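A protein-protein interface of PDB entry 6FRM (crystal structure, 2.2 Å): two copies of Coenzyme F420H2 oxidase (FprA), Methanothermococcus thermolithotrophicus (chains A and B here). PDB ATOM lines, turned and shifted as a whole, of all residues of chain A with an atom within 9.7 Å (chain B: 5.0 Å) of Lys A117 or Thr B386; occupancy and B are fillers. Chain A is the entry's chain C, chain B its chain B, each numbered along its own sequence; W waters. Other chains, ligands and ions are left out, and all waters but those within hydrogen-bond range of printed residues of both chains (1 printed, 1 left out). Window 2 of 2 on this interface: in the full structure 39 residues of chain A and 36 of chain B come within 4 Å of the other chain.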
ATOM      1  N   VAL A  85      12.394  -2.592  14.992  1.00  0.00           N
ATOM      2  CA  VAL A  85      13.491  -3.567  15.042  1.00  0.00           C
ATOM      3  C   VAL A  85      14.362  -3.421  16.291  1.00  0.00           C
ATOM      4  O   VAL A  85      14.886  -4.427  16.762  1.00  0.00           O
ATOM      5  CB  VAL A  85      14.318  -3.505  13.724  1.00  0.00           C
ATOM      6  CG1 VAL A  85      15.653  -4.232  13.832  1.00  0.00           C
ATOM      7  CG2 VAL A  85      13.515  -4.070  12.570  1.00  0.00           C
ATOM      8  N   SER A  90      12.200  -5.439  20.696  1.00  0.00           N
ATOM      9  CA  SER A  90      12.253  -6.714  19.994  1.00  0.00           C
ATOM     10  C   SER A  90      13.131  -7.762  20.675  1.00  0.00           C
ATOM     11  O   SER A  90      13.166  -8.893  20.211  1.00  0.00           O
ATOM     12  CB  SER A  90      12.758  -6.481  18.580  1.00  0.00           C
ATOM     13  OG  SER A  90      14.138  -6.166  18.618  1.00  0.00           O
ATOM     14  N   LEU A  93      11.636 -11.151  21.261  1.00  0.00           N
ATOM     15  CA  LEU A  93      11.041 -11.807  20.087  1.00  0.00           C
ATOM     16  C   LEU A  93      11.534 -13.254  19.909  1.00  0.00           C
ATOM     17  O   LEU A  93      10.685 -14.127  19.711  1.00  0.00           O
ATOM     18  CB  LEU A  93      11.199 -10.974  18.786  1.00  0.00           C
ATOM     19  CG  LEU A  93      10.495 -11.478  17.531  1.00  0.00           C
ATOM     20  CD1 LEU A  93       9.019 -11.711  17.764  1.00  0.00           C
ATOM     21  CD2 LEU A  93      10.685 -10.518  16.376  1.00  0.00           C
ATOM     22  N   PRO A  94      12.856 -13.566  19.988  1.00  0.00           N
ATOM     23  CA  PRO A  94      13.284 -14.975  19.842  1.00  0.00           C
ATOM     24  C   PRO A  94      12.599 -15.924  20.823  1.00  0.00           C
ATOM     25  O   PRO A  94      12.201 -17.016  20.416  1.00  0.00           O
ATOM     26  CB  PRO A  94      14.801 -14.920  20.102  1.00  0.00           C
ATOM     27  CG  PRO A  94      15.176 -13.550  19.854  1.00  0.00           C
ATOM     28  CD  PRO A  94      14.023 -12.681  20.201  1.00  0.00           C
ATOM     29  N   VAL A 110      11.488  -4.169   5.518  1.00  0.00           N
ATOM     30  CA  VAL A 110      12.847  -3.867   5.995  1.00  0.00           C
ATOM     31  C   VAL A 110      13.068  -4.495   7.382  1.00  0.00           C
ATOM     32  O   VAL A 110      14.174  -4.982   7.662  1.00  0.00           O
ATOM     33  CB  VAL A 110      13.142  -2.332   5.964  1.00  0.00           C
ATOM     34  CG1 VAL A 110      14.584  -2.026   6.326  1.00  0.00           C
ATOM     35  CG2 VAL A 110      12.819  -1.747   4.592  1.00  0.00           C
ATOM     36  N   ALA A 111      12.011  -4.484   8.230  1.00  0.00           N
ATOM     37  CA  ALA A 111      12.052  -5.031   9.579  1.00  0.00           C
ATOM     38  C   ALA A 111      12.450  -6.516   9.629  1.00  0.00           C
ATOM     39  O   ALA A 111      13.218  -6.885  10.516  1.00  0.00           O
ATOM     40  CB  ALA A 111      10.739  -4.798  10.300  1.00  0.00           C
ATOM     41  N   VAL A 112      11.965  -7.344   8.665  1.00  0.00           N
ATOM     42  CA  VAL A 112      12.270  -8.781   8.562  1.00  0.00           C
ATOM     43  C   VAL A 112      13.793  -9.014   8.577  1.00  0.00           C
ATOM     44  O   VAL A 112      14.296  -9.783   9.396  1.00  0.00           O
ATOM     45  CB  VAL A 112      11.608  -9.439   7.314  1.00  0.00           C
ATOM     46  CG1 VAL A 112      11.970 -10.918   7.220  1.00  0.00           C
ATOM     47  CG2 VAL A 112      10.091  -9.278   7.338  1.00  0.00           C
ATOM     48  N   GLU A 113      14.510  -8.328   7.676  1.00  0.00           N
ATOM     49  CA  GLU A 113      15.953  -8.409   7.528  1.00  0.00           C
ATOM     50  C   GLU A 113      16.695  -7.973   8.794  1.00  0.00           C
ATOM     51  O   GLU A 113      17.635  -8.659   9.206  1.00  0.00           O
ATOM     52  CB  GLU A 113      16.381  -7.562   6.339  1.00  0.00           C
ATOM     53  CG  GLU A 113      17.802  -7.837   5.890  1.00  0.00           C
ATOM     54  CD  GLU A 113      18.362  -6.812   4.923  1.00  0.00           C
ATOM     55  OE1 GLU A 113      19.580  -6.876   4.641  1.00  0.00           O
ATOM     56  OE2 GLU A 113      17.595  -5.922   4.481  1.00  0.00           O
ATOM     57  N   GLY A 114      16.270  -6.848   9.378  1.00  0.00           N
ATOM     58  CA  GLY A 114      16.846  -6.284  10.596  1.00  0.00           C
ATOM     59  C   GLY A 114      16.669  -7.209  11.782  1.00  0.00           C
ATOM     60  O   GLY A 114      17.614  -7.414  12.546  1.00  0.00           O
ATOM     61  N   LEU A 115      15.459  -7.797  11.927  1.00  0.00           N
ATOM     62  CA  LEU A 115      15.135  -8.718  13.013  1.00  0.00           C
ATOM     63  C   LEU A 115      15.959  -9.998  12.929  1.00  0.00           C
ATOM     64  O   LEU A 115      16.491 -10.441  13.943  1.00  0.00           O
ATOM     65  CB  LEU A 115      13.621  -9.020  13.064  1.00  0.00           C
ATOM     66  CG  LEU A 115      12.732  -7.884  13.602  1.00  0.00           C
ATOM     67  CD1 LEU A 115      11.283  -8.126  13.262  1.00  0.00           C
ATOM     68  CD2 LEU A 115      12.930  -7.674  15.101  1.00  0.00           C
ATOM     69  N   VAL A 116      16.085 -10.577  11.723  1.00  0.00           N
ATOM     70  CA  VAL A 116      16.862 -11.804  11.501  1.00  0.00           C
ATOM     71  C   VAL A 116      18.368 -11.538  11.733  1.00  0.00           C
ATOM     72  O   VAL A 116      19.072 -12.425  12.228  1.00  0.00           O
ATOM     73  CB  VAL A 116      16.553 -12.441  10.114  1.00  0.00           C
ATOM     74  CG1 VAL A 116      17.497 -13.594   9.820  1.00  0.00           C
ATOM     75  CG2 VAL A 116      15.101 -12.915  10.043  1.00  0.00           C
ATOM     76  N   LYS A 117      18.845 -10.319  11.391  1.00  0.00           N
ATOM     77  CA  LYS A 117      20.248  -9.936  11.598  1.00  0.00           C
ATOM     78  C   LYS A 117      20.563  -9.863  13.105  1.00  0.00           C
ATOM     79  O   LYS A 117      21.639 -10.289  13.538  1.00  0.00           O
ATOM     80  CB  LYS A 117      20.587  -8.609  10.904  1.00  0.00           C
ATOM     81  CG  LYS A 117      22.084  -8.395  10.750  1.00  0.00           C
ATOM     82  CD  LYS A 117      22.623  -9.120   9.523  1.00  0.00           C
ATOM     83  CE  LYS A 117      24.026  -9.652   9.655  1.00  0.00           C
ATOM     84  NZ  LYS A 117      25.030  -8.606   9.964  1.00  0.00           N
ATOM     85  N   HIS A 118      19.604  -9.354  13.895  1.00  0.00           N
ATOM     86  CA  HIS A 118      19.700  -9.241  15.354  1.00  0.00           C
ATOM     87  C   HIS A 118      19.580 -10.597  15.994  1.00  0.00           C
ATOM     88  O   HIS A 118      20.326 -10.899  16.922  1.00  0.00           O
ATOM     89  CB  HIS A 118      18.560  -8.385  15.917  1.00  0.00           C
ATOM     90  CG  HIS A 118      18.808  -6.915  15.901  1.00  0.00           C
ATOM     91  ND1 HIS A 118      19.551  -6.301  16.882  1.00  0.00           N
ATOM     92  CD2 HIS A 118      18.361  -5.982  15.034  1.00  0.00           C
ATOM     93  CE1 HIS A 118      19.544  -5.017  16.574  1.00  0.00           C
ATOM     94  NE2 HIS A 118      18.835  -4.780  15.473  1.00  0.00           N
ATOM     95  N   PHE A 119      18.617 -11.411  15.526  1.00  0.00           N
ATOM     96  CA  PHE A 119      18.330 -12.734  16.091  1.00  0.00           C
ATOM     97  C   PHE A 119      18.298 -13.841  15.040  1.00  0.00           C
ATOM     98  O   PHE A 119      17.240 -14.119  14.472  1.00  0.00           O
ATOM     99  CB  PHE A 119      17.025 -12.666  16.909  1.00  0.00           C
ATOM    100  CG  PHE A 119      16.788 -11.359  17.653  1.00  0.00           C
ATOM    101  CD1 PHE A 119      17.535 -11.032  18.788  1.00  0.00           C
ATOM    102  CD2 PHE A 119      15.815 -10.457  17.222  1.00  0.00           C
ATOM    103  CE1 PHE A 119      17.322  -9.823  19.469  1.00  0.00           C
ATOM    104  CE2 PHE A 119      15.592  -9.255  17.916  1.00  0.00           C
ATOM    105  CZ  PHE A 119      16.357  -8.941  19.028  1.00  0.00           C
ATOM    106  N   PRO A 120      19.460 -14.501  14.780  1.00  0.00           N
ATOM    107  CA  PRO A 120      19.509 -15.558  13.750  1.00  0.00           C
ATOM    108  C   PRO A 120      18.520 -16.720  13.903  1.00  0.00           C
ATOM    109  O   PRO A 120      18.206 -17.374  12.904  1.00  0.00           O
ATOM    110  CB  PRO A 120      20.959 -16.046  13.804  1.00  0.00           C
ATOM    111  CG  PRO A 120      21.724 -14.914  14.383  1.00  0.00           C
ATOM    112  CD  PRO A 120      20.799 -14.272  15.368  1.00  0.00           C
ATOM    113  N   SER A 121      18.022 -16.969  15.121  1.00  0.00           N
ATOM    114  CA  SER A 121      17.052 -18.037  15.402  1.00  0.00           C
ATOM    115  C   SER A 121      15.700 -17.768  14.711  1.00  0.00           C
ATOM    116  O   SER A 121      14.888 -18.685  14.566  1.00  0.00           O
ATOM    117  CB  SER A 121      16.860 -18.200  16.909  1.00  0.00           C
ATOM    118  OG  SER A 121      16.257 -17.049  17.468  1.00  0.00           O
ATOM    119  N   LEU A 122      15.481 -16.510  14.278  1.00  0.00           N
ATOM    120  CA  LEU A 122      14.259 -16.078  13.599  1.00  0.00           C
ATOM    121  C   LEU A 122      14.255 -16.413  12.102  1.00  0.00           C
ATOM    122  O   LEU A 122      13.235 -16.209  11.449  1.00  0.00           O
ATOM    123  CB  LEU A 122      13.968 -14.582  13.856  1.00  0.00           C
ATOM    124  CG  LEU A 122      13.701 -14.190  15.322  1.00  0.00           C
ATOM    125  CD1 LEU A 122      13.483 -12.712  15.449  1.00  0.00           C
ATOM    126  CD2 LEU A 122      12.535 -14.955  15.904  1.00  0.00           C
ATOM    127  N   LYS A 123      15.381 -16.935  11.552  1.00  0.00           N
ATOM    128  CA  LYS A 123      15.440 -17.318  10.139  1.00  0.00           C
ATOM    129  C   LYS A 123      14.433 -18.462   9.988  1.00  0.00           C
ATOM    130  O   LYS A 123      14.503 -19.455  10.719  1.00  0.00           O
ATOM    131  CB  LYS A 123      16.858 -17.749   9.706  1.00  0.00           C
ATOM    132  CG  LYS A 123      16.996 -17.785   8.184  1.00  0.00           C
ATOM    133  CD  LYS A 123      18.413 -17.906   7.675  1.00  0.00           C
ATOM    134  CE  LYS A 123      18.369 -18.207   6.195  1.00  0.00           C
ATOM    135  NZ  LYS A 123      19.616 -17.809   5.499  1.00  0.00           N
ATOM    136  N   PHE A 127       7.112 -14.578   9.234  1.00  0.00           N
ATOM    137  CA  PHE A 127       6.940 -13.132   9.109  1.00  0.00           C
ATOM    138  C   PHE A 127       5.822 -12.779   8.124  1.00  0.00           C
ATOM    139  O   PHE A 127       5.659 -13.433   7.088  1.00  0.00           O
ATOM    140  CB  PHE A 127       8.231 -12.459   8.651  1.00  0.00           C
ATOM    141  CG  PHE A 127       9.358 -12.519   9.645  1.00  0.00           C
ATOM    142  CD1 PHE A 127       9.472 -11.570  10.647  1.00  0.00           C
ATOM    143  CD2 PHE A 127      10.318 -13.521   9.570  1.00  0.00           C
ATOM    144  CE1 PHE A 127      10.521 -11.625  11.559  1.00  0.00           C
ATOM    145  CE2 PHE A 127      11.369 -13.574  10.485  1.00  0.00           C
ATOM    146  CZ  PHE A 127      11.466 -12.624  11.468  1.00  0.00           C
ATOM    147  N   TYR B 382      26.001  -4.285   9.100  1.00  0.00           N
ATOM    148  CA  TYR B 382      24.589  -4.127   9.445  1.00  0.00           C
ATOM    149  C   TYR B 382      24.238  -4.833  10.735  1.00  0.00           C
ATOM    150  O   TYR B 382      24.410  -6.042  10.848  1.00  0.00           O
ATOM    151  CB  TYR B 382      23.754  -4.668   8.269  1.00  0.00           C
ATOM    152  CG  TYR B 382      22.251  -4.464   8.296  1.00  0.00           C
ATOM    153  CD1 TYR B 382      21.697  -3.197   8.474  1.00  0.00           C
ATOM    154  CD2 TYR B 382      21.381  -5.528   8.061  1.00  0.00           C
ATOM    155  CE1 TYR B 382      20.315  -3.003   8.453  1.00  0.00           C
ATOM    156  CE2 TYR B 382      20.001  -5.346   8.037  1.00  0.00           C
ATOM    157  CZ  TYR B 382      19.471  -4.085   8.233  1.00  0.00           C
ATOM    158  OH  TYR B 382      18.105  -3.936   8.213  1.00  0.00           O
ATOM    159  N   TYR B 383      23.756  -4.071  11.716  1.00  0.00           N
ATOM    160  CA  TYR B 383      23.343  -4.547  13.028  1.00  0.00           C
ATOM    161  C   TYR B 383      24.342  -5.514  13.690  1.00  0.00           C
ATOM    162  O   TYR B 383      25.522  -5.195  13.769  1.00  0.00           O
ATOM    163  CB  TYR B 383      21.925  -5.133  12.982  1.00  0.00           C
ATOM    164  CG  TYR B 383      20.843  -4.098  12.753  1.00  0.00           C
ATOM    165  CD1 TYR B 383      20.756  -2.957  13.548  1.00  0.00           C
ATOM    166  CD2 TYR B 383      19.881  -4.276  11.769  1.00  0.00           C
ATOM    167  CE1 TYR B 383      19.745  -2.011  13.354  1.00  0.00           C
ATOM    168  CE2 TYR B 383      18.866  -3.343  11.569  1.00  0.00           C
ATOM    169  CZ  TYR B 383      18.803  -2.208  12.359  1.00  0.00           C
ATOM    170  OH  TYR B 383      17.807  -1.291  12.132  1.00  0.00           O
ATOM    171  N   VAL B 384      23.872  -6.674  14.158  1.00  0.00           N
ATOM    172  CA  VAL B 384      24.677  -7.676  14.865  1.00  0.00           C
ATOM    173  C   VAL B 384      25.622  -8.425  13.914  1.00  0.00           C
ATOM    174  O   VAL B 384      25.149  -8.954  12.906  1.00  0.00           O
ATOM    175  CB  VAL B 384      23.781  -8.619  15.711  1.00  0.00           C
ATOM    176  CG1 VAL B 384      24.611  -9.590  16.539  1.00  0.00           C
ATOM    177  CG2 VAL B 384      22.852  -7.815  16.622  1.00  0.00           C
ATOM    178  N   PRO B 385      26.953  -8.474  14.215  1.00  0.00           N
ATOM    179  CA  PRO B 385      27.875  -9.196  13.324  1.00  0.00           C
ATOM    180  C   PRO B 385      27.631 -10.705  13.318  1.00  0.00           C
ATOM    181  O   PRO B 385      27.359 -11.288  14.368  1.00  0.00           O
ATOM    182  CB  PRO B 385      29.268  -8.889  13.895  1.00  0.00           C
ATOM    183  CG  PRO B 385      29.076  -7.841  14.924  1.00  0.00           C
ATOM    184  CD  PRO B 385      27.669  -7.900  15.378  1.00  0.00           C
ATOM    185  N   THR B 386      27.741 -11.340  12.148  1.00  0.00           N
ATOM    186  CA  THR B 386      27.570 -12.799  12.068  1.00  0.00           C
ATOM    187  C   THR B 386      28.945 -13.399  12.398  1.00  0.00           C
ATOM    188  O   THR B 386      29.928 -12.656  12.533  1.00  0.00           O
ATOM    189  CB  THR B 386      27.179 -13.238  10.647  1.00  0.00           C
ATOM    190  OG1 THR B 386      28.224 -12.885   9.736  1.00  0.00           O
ATOM    191  CG2 THR B 386      25.854 -12.666  10.198  1.00  0.00           C
ATOM    192  N   GLU B 387      29.026 -14.731  12.491  1.00  0.00           N
ATOM    193  CA  GLU B 387      30.282 -15.424  12.758  1.00  0.00           C
ATOM    194  C   GLU B 387      31.304 -15.087  11.661  1.00  0.00           C
ATOM    195  O   GLU B 387      32.461 -14.815  11.971  1.00  0.00           O
ATOM    196  CB  GLU B 387      30.057 -16.931  12.837  1.00  0.00           C
ATOM    197  CG  GLU B 387      31.077 -17.584  13.748  1.00  0.00           C
ATOM    198  CD  GLU B 387      30.690 -17.635  15.214  1.00  0.00           C
ATOM    199  OE1 GLU B 387      30.427 -16.567  15.817  1.00  0.00           O
ATOM    200  OE2 GLU B 387      30.688 -18.757  15.770  1.00  0.00           O
ATOM    201  N   ASP B 388      30.857 -15.077  10.386  1.00  0.00           N
ATOM    202  CA  ASP B 388      31.679 -14.761   9.219  1.00  0.00           C
ATOM    203  C   ASP B 388      32.197 -13.325   9.261  1.00  0.00           C
ATOM    204  O   ASP B 388      33.355 -13.085   8.899  1.00  0.00           O
ATOM    205  CB  ASP B 388      30.921 -15.028   7.911  1.00  0.00           C
ATOM    206  CG  ASP B 388      30.738 -16.499   7.564  1.00  0.00           C
ATOM    207  OD1 ASP B 388      31.352 -17.362   8.244  1.00  0.00           O
ATOM    208  OD2 ASP B 388      30.021 -16.786   6.591  1.00  0.00           O
ATOM    209  N   GLU B 389      31.354 -12.378   9.710  1.00  0.00           N
ATOM    210  CA  GLU B 389      31.734 -10.969   9.829  1.00  0.00           C
ATOM    211  C   GLU B 389      32.792 -10.791  10.917  1.00  0.00           C
ATOM    212  O   GLU B 389      33.714 -10.022  10.731  1.00  0.00           O
ATOM    213  CB  GLU B 389      30.505 -10.089  10.048  1.00  0.00           C
ATOM    214  CG  GLU B 389      29.646  -9.986   8.799  1.00  0.00           C
ATOM    215  CD  GLU B 389      28.297  -9.316   8.953  1.00  0.00           C
ATOM    216  OE1 GLU B 389      27.712  -9.362  10.060  1.00  0.00           O
ATOM    217  OE2 GLU B 389      27.803  -8.776   7.940  1.00  0.00           O
ATOM    218  N   LEU B 390      32.679 -11.531  12.032  1.00  0.00           N
ATOM    219  CA  LEU B 390      33.661 -11.479  13.123  1.00  0.00           C
ATOM    220  C   LEU B 390      35.008 -12.081  12.672  1.00  0.00           C
ATOM    221  O   LEU B 390      36.066 -11.610  13.109  1.00  0.00           O
ATOM    222  CB  LEU B 390      33.144 -12.159  14.402  1.00  0.00           C
ATOM    223  CG  LEU B 390      31.985 -11.445  15.137  1.00  0.00           C
ATOM    224  CD1 LEU B 390      31.471 -12.284  16.265  1.00  0.00           C
ATOM    225  CD2 LEU B 390      32.391 -10.050  15.649  1.00  0.00           C
HETATM  226  O   HOH W   1      26.186  -6.761   7.414  1.00  0.00           O
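Water W1 lies within hydrogen-bond range of OE2 of Glu B389 (2.6 Å), N of Tyr B382 (3.0 Å) and NZ of Lys A117 (3.4 Å).
Hydrophobic or aromatic side chains of chain B that line the printed part of chain A: Tyr B382, Tyr B383 and Val B384. Hydrophobic or aromatic side chains of chain A that line the printed part of chain B: His A118. Among the printed residues, 10 pairs touch across the chains. Among the printed residues, Asp or Glu carboxylates within 4 Å of a Lys or Arg side-chain nitrogen of the other chain: Lys A117 with Glu B389.
Lys A117 touches just these residues of chain B: Tyr B382 (2.8 Å), Tyr B383 (3.96 Å), Val B384 (3.0 Å), Thr B386 (3.6 Å) and Glu B389 (2.8 Å). Of chain A, only Lys A117 (3.6 Å) comes within 4 Å of Thr B386. Val B384 touches just these residues of chain A: Lys A117 and His A118. No residue of chain A comes within 4 Å of Pro B385. Printed residues of chain A within 4 Å of Tyr B383: Gly A114 (3.7 Å), Lys A117 (3.96 Å) and His A118 (3.3 Å). Printed residues of chain B within 4 Å of Glu A113: Tyr B382 (3.7 Å). Of the printed residues of chain B, Gly A114 touches Tyr B382 (3.6 Å) and Tyr B383 (3.7 Å). Of the printed residues of chain B, His A118 touches Tyr B383 and Val B384. Of the printed residues of chain A, Tyr B382 touches Glu A113 (3.7 Å), Gly A114 (3.6 Å) and Lys A117 (2.8 Å). Val A116 touches none of the printed residues of chain B. Leu A93 touches none of the printed residues of chain B.
CE2 of Tyr B382 touches OE1 of Glu A113, 3.7 Å away. Tyr B382 touches Gly A114 (OH to CA, 3.6 Å). CE2 of Tyr B383 touches CA of Gly A114, at 3.7 Å. Lys A117 touches Tyr B383 (CG to CB, 3.96 Å). CE of Lys A117 touches CG2 of Thr B386, at 3.6 Å. Tyr B383 touches His A118 (CD1 to NE2, 3.3 Å). His A118 touches Val B384.
No position is printed for both chains. Of the 10 pairs that touch across the chains among the printed residues, none has its exchanged pair printed and touching as well.
The side-chain hydroxyl (OG1) of Thr B386 lies close to the backbone NH (N) of Asp B388. The side-chain carboxylate of Glu B389 lies within hydrogen-bond range of the backbone NH of Thr B386, at 2.9 Å.
NZ of Lys A117 lies within hydrogen-bond range of O of Tyr B382, at 2.8 Å. NZ of Lys A117 lies within hydrogen-bond range of O of Val B384, at 3.0 Å. The side-chain carboxylate (OE1) of Glu B389 is in salt-bridge range of the side-chain amino group (NZ) of Lys A117 (2.8 Å).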
